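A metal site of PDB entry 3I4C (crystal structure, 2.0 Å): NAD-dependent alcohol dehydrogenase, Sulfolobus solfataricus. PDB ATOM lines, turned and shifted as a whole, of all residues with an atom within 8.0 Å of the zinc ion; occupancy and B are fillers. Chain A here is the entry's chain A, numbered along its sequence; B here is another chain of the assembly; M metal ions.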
ATOM      1  N   GLN A  96     -11.668 -17.513  14.553  1.00  0.00           N
ATOM      2  CA  GLN A  96     -12.906 -16.778  14.334  1.00  0.00           C
ATOM      3  C   GLN A  96     -12.825 -15.611  13.354  1.00  0.00           C
ATOM      4  O   GLN A  96     -12.107 -14.632  13.590  1.00  0.00           O
ATOM      5  CB  GLN A  96     -13.388 -16.333  15.724  1.00  0.00           C
ATOM      6  CG  GLN A  96     -13.326 -17.523  16.695  1.00  0.00           C
ATOM      7  CD  GLN A  96     -13.526 -17.172  18.160  1.00  0.00           C
ATOM      8  OE1 GLN A  96     -13.772 -16.020  18.511  1.00  0.00           O
ATOM      9  NE2 GLN A  96     -13.418 -18.174  19.029  1.00  0.00           N
ATOM     10  N   GLY A  97     -13.552 -15.719  12.252  1.00  0.00           N
ATOM     11  CA  GLY A  97     -13.524 -14.695  11.216  1.00  0.00           C
ATOM     12  C   GLY A  97     -14.178 -13.362  11.536  1.00  0.00           C
ATOM     13  O   GLY A  97     -15.104 -13.275  12.347  1.00  0.00           O
ATOM     14  N   GLU A  98     -13.687 -12.305  10.882  1.00  0.00           N
ATOM     15  CA  GLU A  98     -14.221 -10.967  11.103  1.00  0.00           C
ATOM     16  C   GLU A  98     -15.593 -10.804  10.434  1.00  0.00           C
ATOM     17  O   GLU A  98     -16.386  -9.939  10.827  1.00  0.00           O
ATOM     18  CB  GLU A  98     -13.228  -9.901  10.632  1.00  0.00           C
ATOM     19  CG  GLU A  98     -12.626 -10.123   9.246  1.00  0.00           C
ATOM     20  CD  GLU A  98     -13.625  -9.933   8.144  1.00  0.00           C
ATOM     21  OE1 GLU A  98     -14.325  -8.907   8.139  1.00  0.00           O
ATOM     22  OE2 GLU A  98     -13.717 -10.806   7.251  1.00  0.00           O
ATOM     23  N   GLY A  99     -15.868 -11.641   9.438  1.00  0.00           N
ATOM     24  CA  GLY A  99     -17.185 -11.618   8.800  1.00  0.00           C
ATOM     25  C   GLY A  99     -17.406 -10.944   7.457  1.00  0.00           C
ATOM     26  O   GLY A  99     -18.245 -11.387   6.677  1.00  0.00           O
ATOM     27  N   ASN A 100     -16.654  -9.883   7.175  1.00  0.00           N
ATOM     28  CA  ASN A 100     -16.834  -9.128   5.931  1.00  0.00           C
ATOM     29  C   ASN A 100     -16.149  -9.700   4.697  1.00  0.00           C
ATOM     30  O   ASN A 100     -16.673  -9.563   3.587  1.00  0.00           O
ATOM     31  CB  ASN A 100     -16.367  -7.679   6.122  1.00  0.00           C
ATOM     32  CG  ASN A 100     -16.660  -6.803   4.922  1.00  0.00           C
ATOM     33  OD1 ASN A 100     -17.821  -6.626   4.538  1.00  0.00           O
ATOM     34  ND2 ASN A 100     -15.609  -6.263   4.304  1.00  0.00           N
ATOM     35  N   CYS A 101     -15.000 -10.348   4.875  1.00  0.00           N
ATOM     36  CA  CYS A 101     -14.274 -10.868   3.730  1.00  0.00           C
ATOM     37  C   CYS A 101     -14.988 -12.000   2.997  1.00  0.00           C
ATOM     38  O   CYS A 101     -15.955 -12.580   3.498  1.00  0.00           O
ATOM     39  CB  CYS A 101     -12.848 -11.292   4.131  1.00  0.00           C
ATOM     40  SG  CYS A 101     -12.632 -12.957   4.860  1.00  0.00           S
ATOM     41  N   TYR A 102     -14.496 -12.292   1.799  1.00  0.00           N
ATOM     42  CA  TYR A 102     -15.047 -13.340   0.945  1.00  0.00           C
ATOM     43  C   TYR A 102     -15.158 -14.700   1.639  1.00  0.00           C
ATOM     44  O   TYR A 102     -16.199 -15.350   1.583  1.00  0.00           O
ATOM     45  CB  TYR A 102     -14.159 -13.494  -0.296  1.00  0.00           C
ATOM     46  CG  TYR A 102     -14.506 -14.710  -1.134  1.00  0.00           C
ATOM     47  CD1 TYR A 102     -15.523 -14.671  -2.082  1.00  0.00           C
ATOM     48  CD2 TYR A 102     -13.811 -15.918  -0.950  1.00  0.00           C
ATOM     49  CE1 TYR A 102     -15.858 -15.801  -2.824  1.00  0.00           C
ATOM     50  CE2 TYR A 102     -14.139 -17.042  -1.688  1.00  0.00           C
ATOM     51  CZ  TYR A 102     -15.161 -16.987  -2.622  1.00  0.00           C
ATOM     52  OH  TYR A 102     -15.480 -18.112  -3.350  1.00  0.00           O
ATOM     53  N   TYR A 103     -14.085 -15.126   2.293  1.00  0.00           N
ATOM     54  CA  TYR A 103     -14.070 -16.421   2.949  1.00  0.00           C
ATOM     55  C   TYR A 103     -15.057 -16.512   4.086  1.00  0.00           C
ATOM     56  O   TYR A 103     -15.645 -17.563   4.317  1.00  0.00           O
ATOM     57  CB  TYR A 103     -12.641 -16.739   3.398  1.00  0.00           C
ATOM     58  CG  TYR A 103     -11.766 -16.854   2.179  1.00  0.00           C
ATOM     59  CD1 TYR A 103     -11.797 -17.992   1.368  1.00  0.00           C
ATOM     60  CD2 TYR A 103     -11.005 -15.770   1.743  1.00  0.00           C
ATOM     61  CE1 TYR A 103     -11.117 -18.034   0.157  1.00  0.00           C
ATOM     62  CE2 TYR A 103     -10.325 -15.800   0.541  1.00  0.00           C
ATOM     63  CZ  TYR A 103     -10.388 -16.941  -0.252  1.00  0.00           C
ATOM     64  OH  TYR A 103      -9.745 -16.938  -1.458  1.00  0.00           O
ATOM     65  N   CYS A 104     -15.250 -15.408   4.794  1.00  0.00           N
ATOM     66  CA  CYS A 104     -16.221 -15.384   5.878  1.00  0.00           C
ATOM     67  C   CYS A 104     -17.620 -15.471   5.283  1.00  0.00           C
ATOM     68  O   CYS A 104     -18.471 -16.176   5.802  1.00  0.00           O
ATOM     69  CB  CYS A 104     -16.068 -14.097   6.695  1.00  0.00           C
ATOM     70  SG  CYS A 104     -14.701 -14.144   7.896  1.00  0.00           S
ATOM     71  N   ARG A 105     -17.847 -14.768   4.176  1.00  0.00           N
ATOM     72  CA  ARG A 105     -19.172 -14.800   3.561  1.00  0.00           C
ATOM     73  C   ARG A 105     -19.565 -16.173   3.010  1.00  0.00           C
ATOM     74  O   ARG A 105     -20.724 -16.559   3.093  1.00  0.00           O
ATOM     75  CB  ARG A 105     -19.280 -13.745   2.446  1.00  0.00           C
ATOM     76  CG  ARG A 105     -19.103 -12.330   2.957  1.00  0.00           C
ATOM     77  CD  ARG A 105     -19.553 -11.305   1.939  1.00  0.00           C
ATOM     78  NE  ARG A 105     -19.206  -9.959   2.371  1.00  0.00           N
ATOM     79  CZ  ARG A 105     -20.012  -8.905   2.252  1.00  0.00           C
ATOM     80  NH1 ARG A 105     -21.213  -9.037   1.712  1.00  0.00           N
ATOM     81  NH2 ARG A 105     -19.591  -7.712   2.661  1.00  0.00           N
ATOM     82  N   GLU A 108     -16.177 -20.099   5.051  1.00  0.00           N
ATOM     83  CA  GLU A 108     -14.864 -20.707   5.242  1.00  0.00           C
ATOM     84  C   GLU A 108     -14.040 -19.742   6.077  1.00  0.00           C
ATOM     85  O   GLU A 108     -12.935 -19.358   5.701  1.00  0.00           O
ATOM     86  CB  GLU A 108     -14.201 -20.934   3.879  1.00  0.00           C
ATOM     87  CG  GLU A 108     -14.977 -21.836   2.915  1.00  0.00           C
ATOM     88  CD  GLU A 108     -14.983 -23.290   3.352  1.00  0.00           C
ATOM     89  OE1 GLU A 108     -13.934 -23.787   3.794  1.00  0.00           O
ATOM     90  OE2 GLU A 108     -16.045 -23.954   3.249  1.00  0.00           O
ATOM     91  N   GLU A 109     -14.578 -19.367   7.235  1.00  0.00           N
ATOM     92  CA  GLU A 109     -13.940 -18.373   8.079  1.00  0.00           C
ATOM     93  C   GLU A 109     -12.537 -18.670   8.550  1.00  0.00           C
ATOM     94  O   GLU A 109     -11.828 -17.749   8.937  1.00  0.00           O
ATOM     95  CB  GLU A 109     -14.813 -18.042   9.281  1.00  0.00           C
ATOM     96  CG  GLU A 109     -14.911 -19.133  10.315  1.00  0.00           C
ATOM     97  CD  GLU A 109     -15.867 -18.756  11.413  1.00  0.00           C
ATOM     98  OE1 GLU A 109     -15.643 -17.709  12.069  1.00  0.00           O
ATOM     99  OE2 GLU A 109     -16.848 -19.493  11.616  1.00  0.00           O
ATOM    100  N   HIS A 110     -12.123 -19.942   8.540  1.00  0.00           N
ATOM    101  CA  HIS A 110     -10.757 -20.247   8.959  1.00  0.00           C
ATOM    102  C   HIS A 110      -9.771 -19.646   7.959  1.00  0.00           C
ATOM    103  O   HIS A 110      -8.577 -19.512   8.238  1.00  0.00           O
ATOM    104  CB  HIS A 110     -10.541 -21.761   9.065  1.00  0.00           C
ATOM    105  CG  HIS A 110     -10.773 -22.493   7.791  1.00  0.00           C
ATOM    106  ND1 HIS A 110     -11.992 -22.538   7.169  1.00  0.00           N
ATOM    107  CD2 HIS A 110      -9.927 -23.223   7.013  1.00  0.00           C
ATOM    108  CE1 HIS A 110     -11.897 -23.250   6.057  1.00  0.00           C
ATOM    109  NE2 HIS A 110     -10.656 -23.675   5.940  1.00  0.00           N
ATOM    110  N   LEU A 111     -10.261 -19.299   6.766  1.00  0.00           N
ATOM    111  CA  LEU A 111      -9.376 -18.706   5.765  1.00  0.00           C
ATOM    112  C   LEU A 111      -9.611 -17.198   5.712  1.00  0.00           C
ATOM    113  O   LEU A 111      -9.247 -16.538   4.740  1.00  0.00           O
ATOM    114  CB  LEU A 111      -9.630 -19.333   4.385  1.00  0.00           C
ATOM    115  CG  LEU A 111      -9.393 -20.844   4.317  1.00  0.00           C
ATOM    116  CD1 LEU A 111      -9.698 -21.372   2.912  1.00  0.00           C
ATOM    117  CD2 LEU A 111      -7.947 -21.172   4.688  1.00  0.00           C
ATOM    118  N   CYS A 112     -10.193 -16.661   6.776  1.00  0.00           N
ATOM    119  CA  CYS A 112     -10.478 -15.230   6.879  1.00  0.00           C
ATOM    120  C   CYS A 112      -9.241 -14.386   6.609  1.00  0.00           C
ATOM    121  O   CYS A 112      -8.135 -14.756   7.000  1.00  0.00           O
ATOM    122  CB  CYS A 112     -10.997 -14.896   8.276  1.00  0.00           C
ATOM    123  SG  CYS A 112     -11.260 -13.103   8.571  1.00  0.00           S
ATOM    124  N   ASP A 113      -9.428 -13.236   5.958  1.00  0.00           N
ATOM    125  CA  ASP A 113      -8.313 -12.325   5.663  1.00  0.00           C
ATOM    126  C   ASP A 113      -7.727 -11.696   6.926  1.00  0.00           C
ATOM    127  O   ASP A 113      -6.541 -11.351   6.948  1.00  0.00           O
ATOM    128  CB  ASP A 113      -8.760 -11.197   4.731  1.00  0.00           C
ATOM    129  CG  ASP A 113      -9.054 -11.673   3.327  1.00  0.00           C
ATOM    130  OD1 ASP A 113      -8.478 -12.700   2.922  1.00  0.00           O
ATOM    131  OD2 ASP A 113      -9.850 -11.009   2.631  1.00  0.00           O
ATOM    132  N   SER A 114      -8.543 -11.511   7.954  1.00  0.00           N
ATOM    133  CA  SER A 114      -8.085 -10.920   9.210  1.00  0.00           C
ATOM    134  C   SER A 114      -8.821 -11.583  10.360  1.00  0.00           C
ATOM    135  O   SER A 114      -9.668 -10.982  11.004  1.00  0.00           O
ATOM    136  CB  SER A 114      -8.375  -9.424   9.211  1.00  0.00           C
ATOM    137  OG  SER A 114      -7.814  -8.803   8.075  1.00  0.00           O
ATOM    138  N   PRO A 115      -8.474 -12.833  10.645  1.00  0.00           N
ATOM    139  CA  PRO A 115      -9.110 -13.597  11.717  1.00  0.00           C
ATOM    140  C   PRO A 115      -8.723 -13.218  13.140  1.00  0.00           C
ATOM    141  O   PRO A 115      -7.685 -12.605  13.388  1.00  0.00           O
ATOM    142  CB  PRO A 115      -8.712 -15.024  11.384  1.00  0.00           C
ATOM    143  CG  PRO A 115      -7.309 -14.845  10.935  1.00  0.00           C
ATOM    144  CD  PRO A 115      -7.391 -13.631  10.026  1.00  0.00           C
ATOM    145  N   ARG A 116      -9.596 -13.589  14.060  1.00  0.00           N
ATOM    146  CA  ARG A 116      -9.373 -13.412  15.479  1.00  0.00           C
ATOM    147  C   ARG A 116      -9.005 -14.853  15.838  1.00  0.00           C
ATOM    148  O   ARG A 116      -9.844 -15.749  15.761  1.00  0.00           O
ATOM    149  CB  ARG A 116     -10.659 -13.011  16.190  1.00  0.00           C
ATOM    150  CG  ARG A 116     -10.504 -12.901  17.699  1.00  0.00           C
ATOM    151  CD  ARG A 116     -10.433 -11.449  18.143  1.00  0.00           C
ATOM    152  NE  ARG A 116     -11.661 -10.728  17.805  1.00  0.00           N
ATOM    153  CZ  ARG A 116     -11.868  -9.438  18.039  1.00  0.00           C
ATOM    154  NH1 ARG A 116     -10.925  -8.704  18.619  1.00  0.00           N
ATOM    155  NH2 ARG A 116     -13.028  -8.881  17.682  1.00  0.00           N
ATOM    156  N   LYS B 263      -6.989 -17.928  -1.941  1.00  0.00           N
ATOM    157  CA  LYS B 263      -7.071 -19.065  -1.042  1.00  0.00           C
ATOM    158  C   LYS B 263      -8.162 -19.979  -1.610  1.00  0.00           C
ATOM    159  O   LYS B 263      -9.167 -19.502  -2.143  1.00  0.00           O
ATOM    160  CB  LYS B 263      -7.397 -18.600   0.386  1.00  0.00           C
ATOM    161  CG  LYS B 263      -6.145 -18.066   1.132  1.00  0.00           C
ATOM    162  CD  LYS B 263      -6.477 -17.361   2.457  1.00  0.00           C
ATOM    163  CE  LYS B 263      -7.102 -16.002   2.214  1.00  0.00           C
ATOM    164  NZ  LYS B 263      -7.287 -15.182   3.460  1.00  0.00           N
HETATM  165 ZN    ZN M   1     -13.023 -12.764   7.088  1.00  0.00          ZN
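Gly 99 touches the zinc ion (N to ZN, 3.9 Å).
Asp 113 touches the zinc ion.
Six residues have an atom within 4 Å of the zinc ion: Glu 98, Gly 99, Cys 101, Cys 104, Cys 112 and Asp 113.
The nearest printed residue that does not touch the zinc ion is Gly 97 (4.6 Å).
The zinc ion is bound by OE2 of Glu 98 (2.1 Å), SG of Cys 101 (2.3 Å), SG of Cys 104 (2.3 Å) and SG of Cys 112 (2.3 Å).
The zinc ion has four donor atoms within binding distance.
N of Asn 100 is in hydrogen-bond range of OE1 of Glu 98, at 2.7 Å.
The side-chain sulfur (SG) of Cys 101 sits close to the backbone NH (N) of Asp 113 (3.4 Å).
The backbone NH (N) of Tyr 103 lies close to the side-chain sulfur (SG) of Cys 101 (3.7 Å).
SG of Cys 104 sits close to N of Gly 99 (3.2 Å).
SG of Cys 112 sits close to N of Ser 114.
The side-chain amino group of Lys 263 of chain B is in salt-bridge range of the side-chain carboxylate of Asp 113 (2.8 Å).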
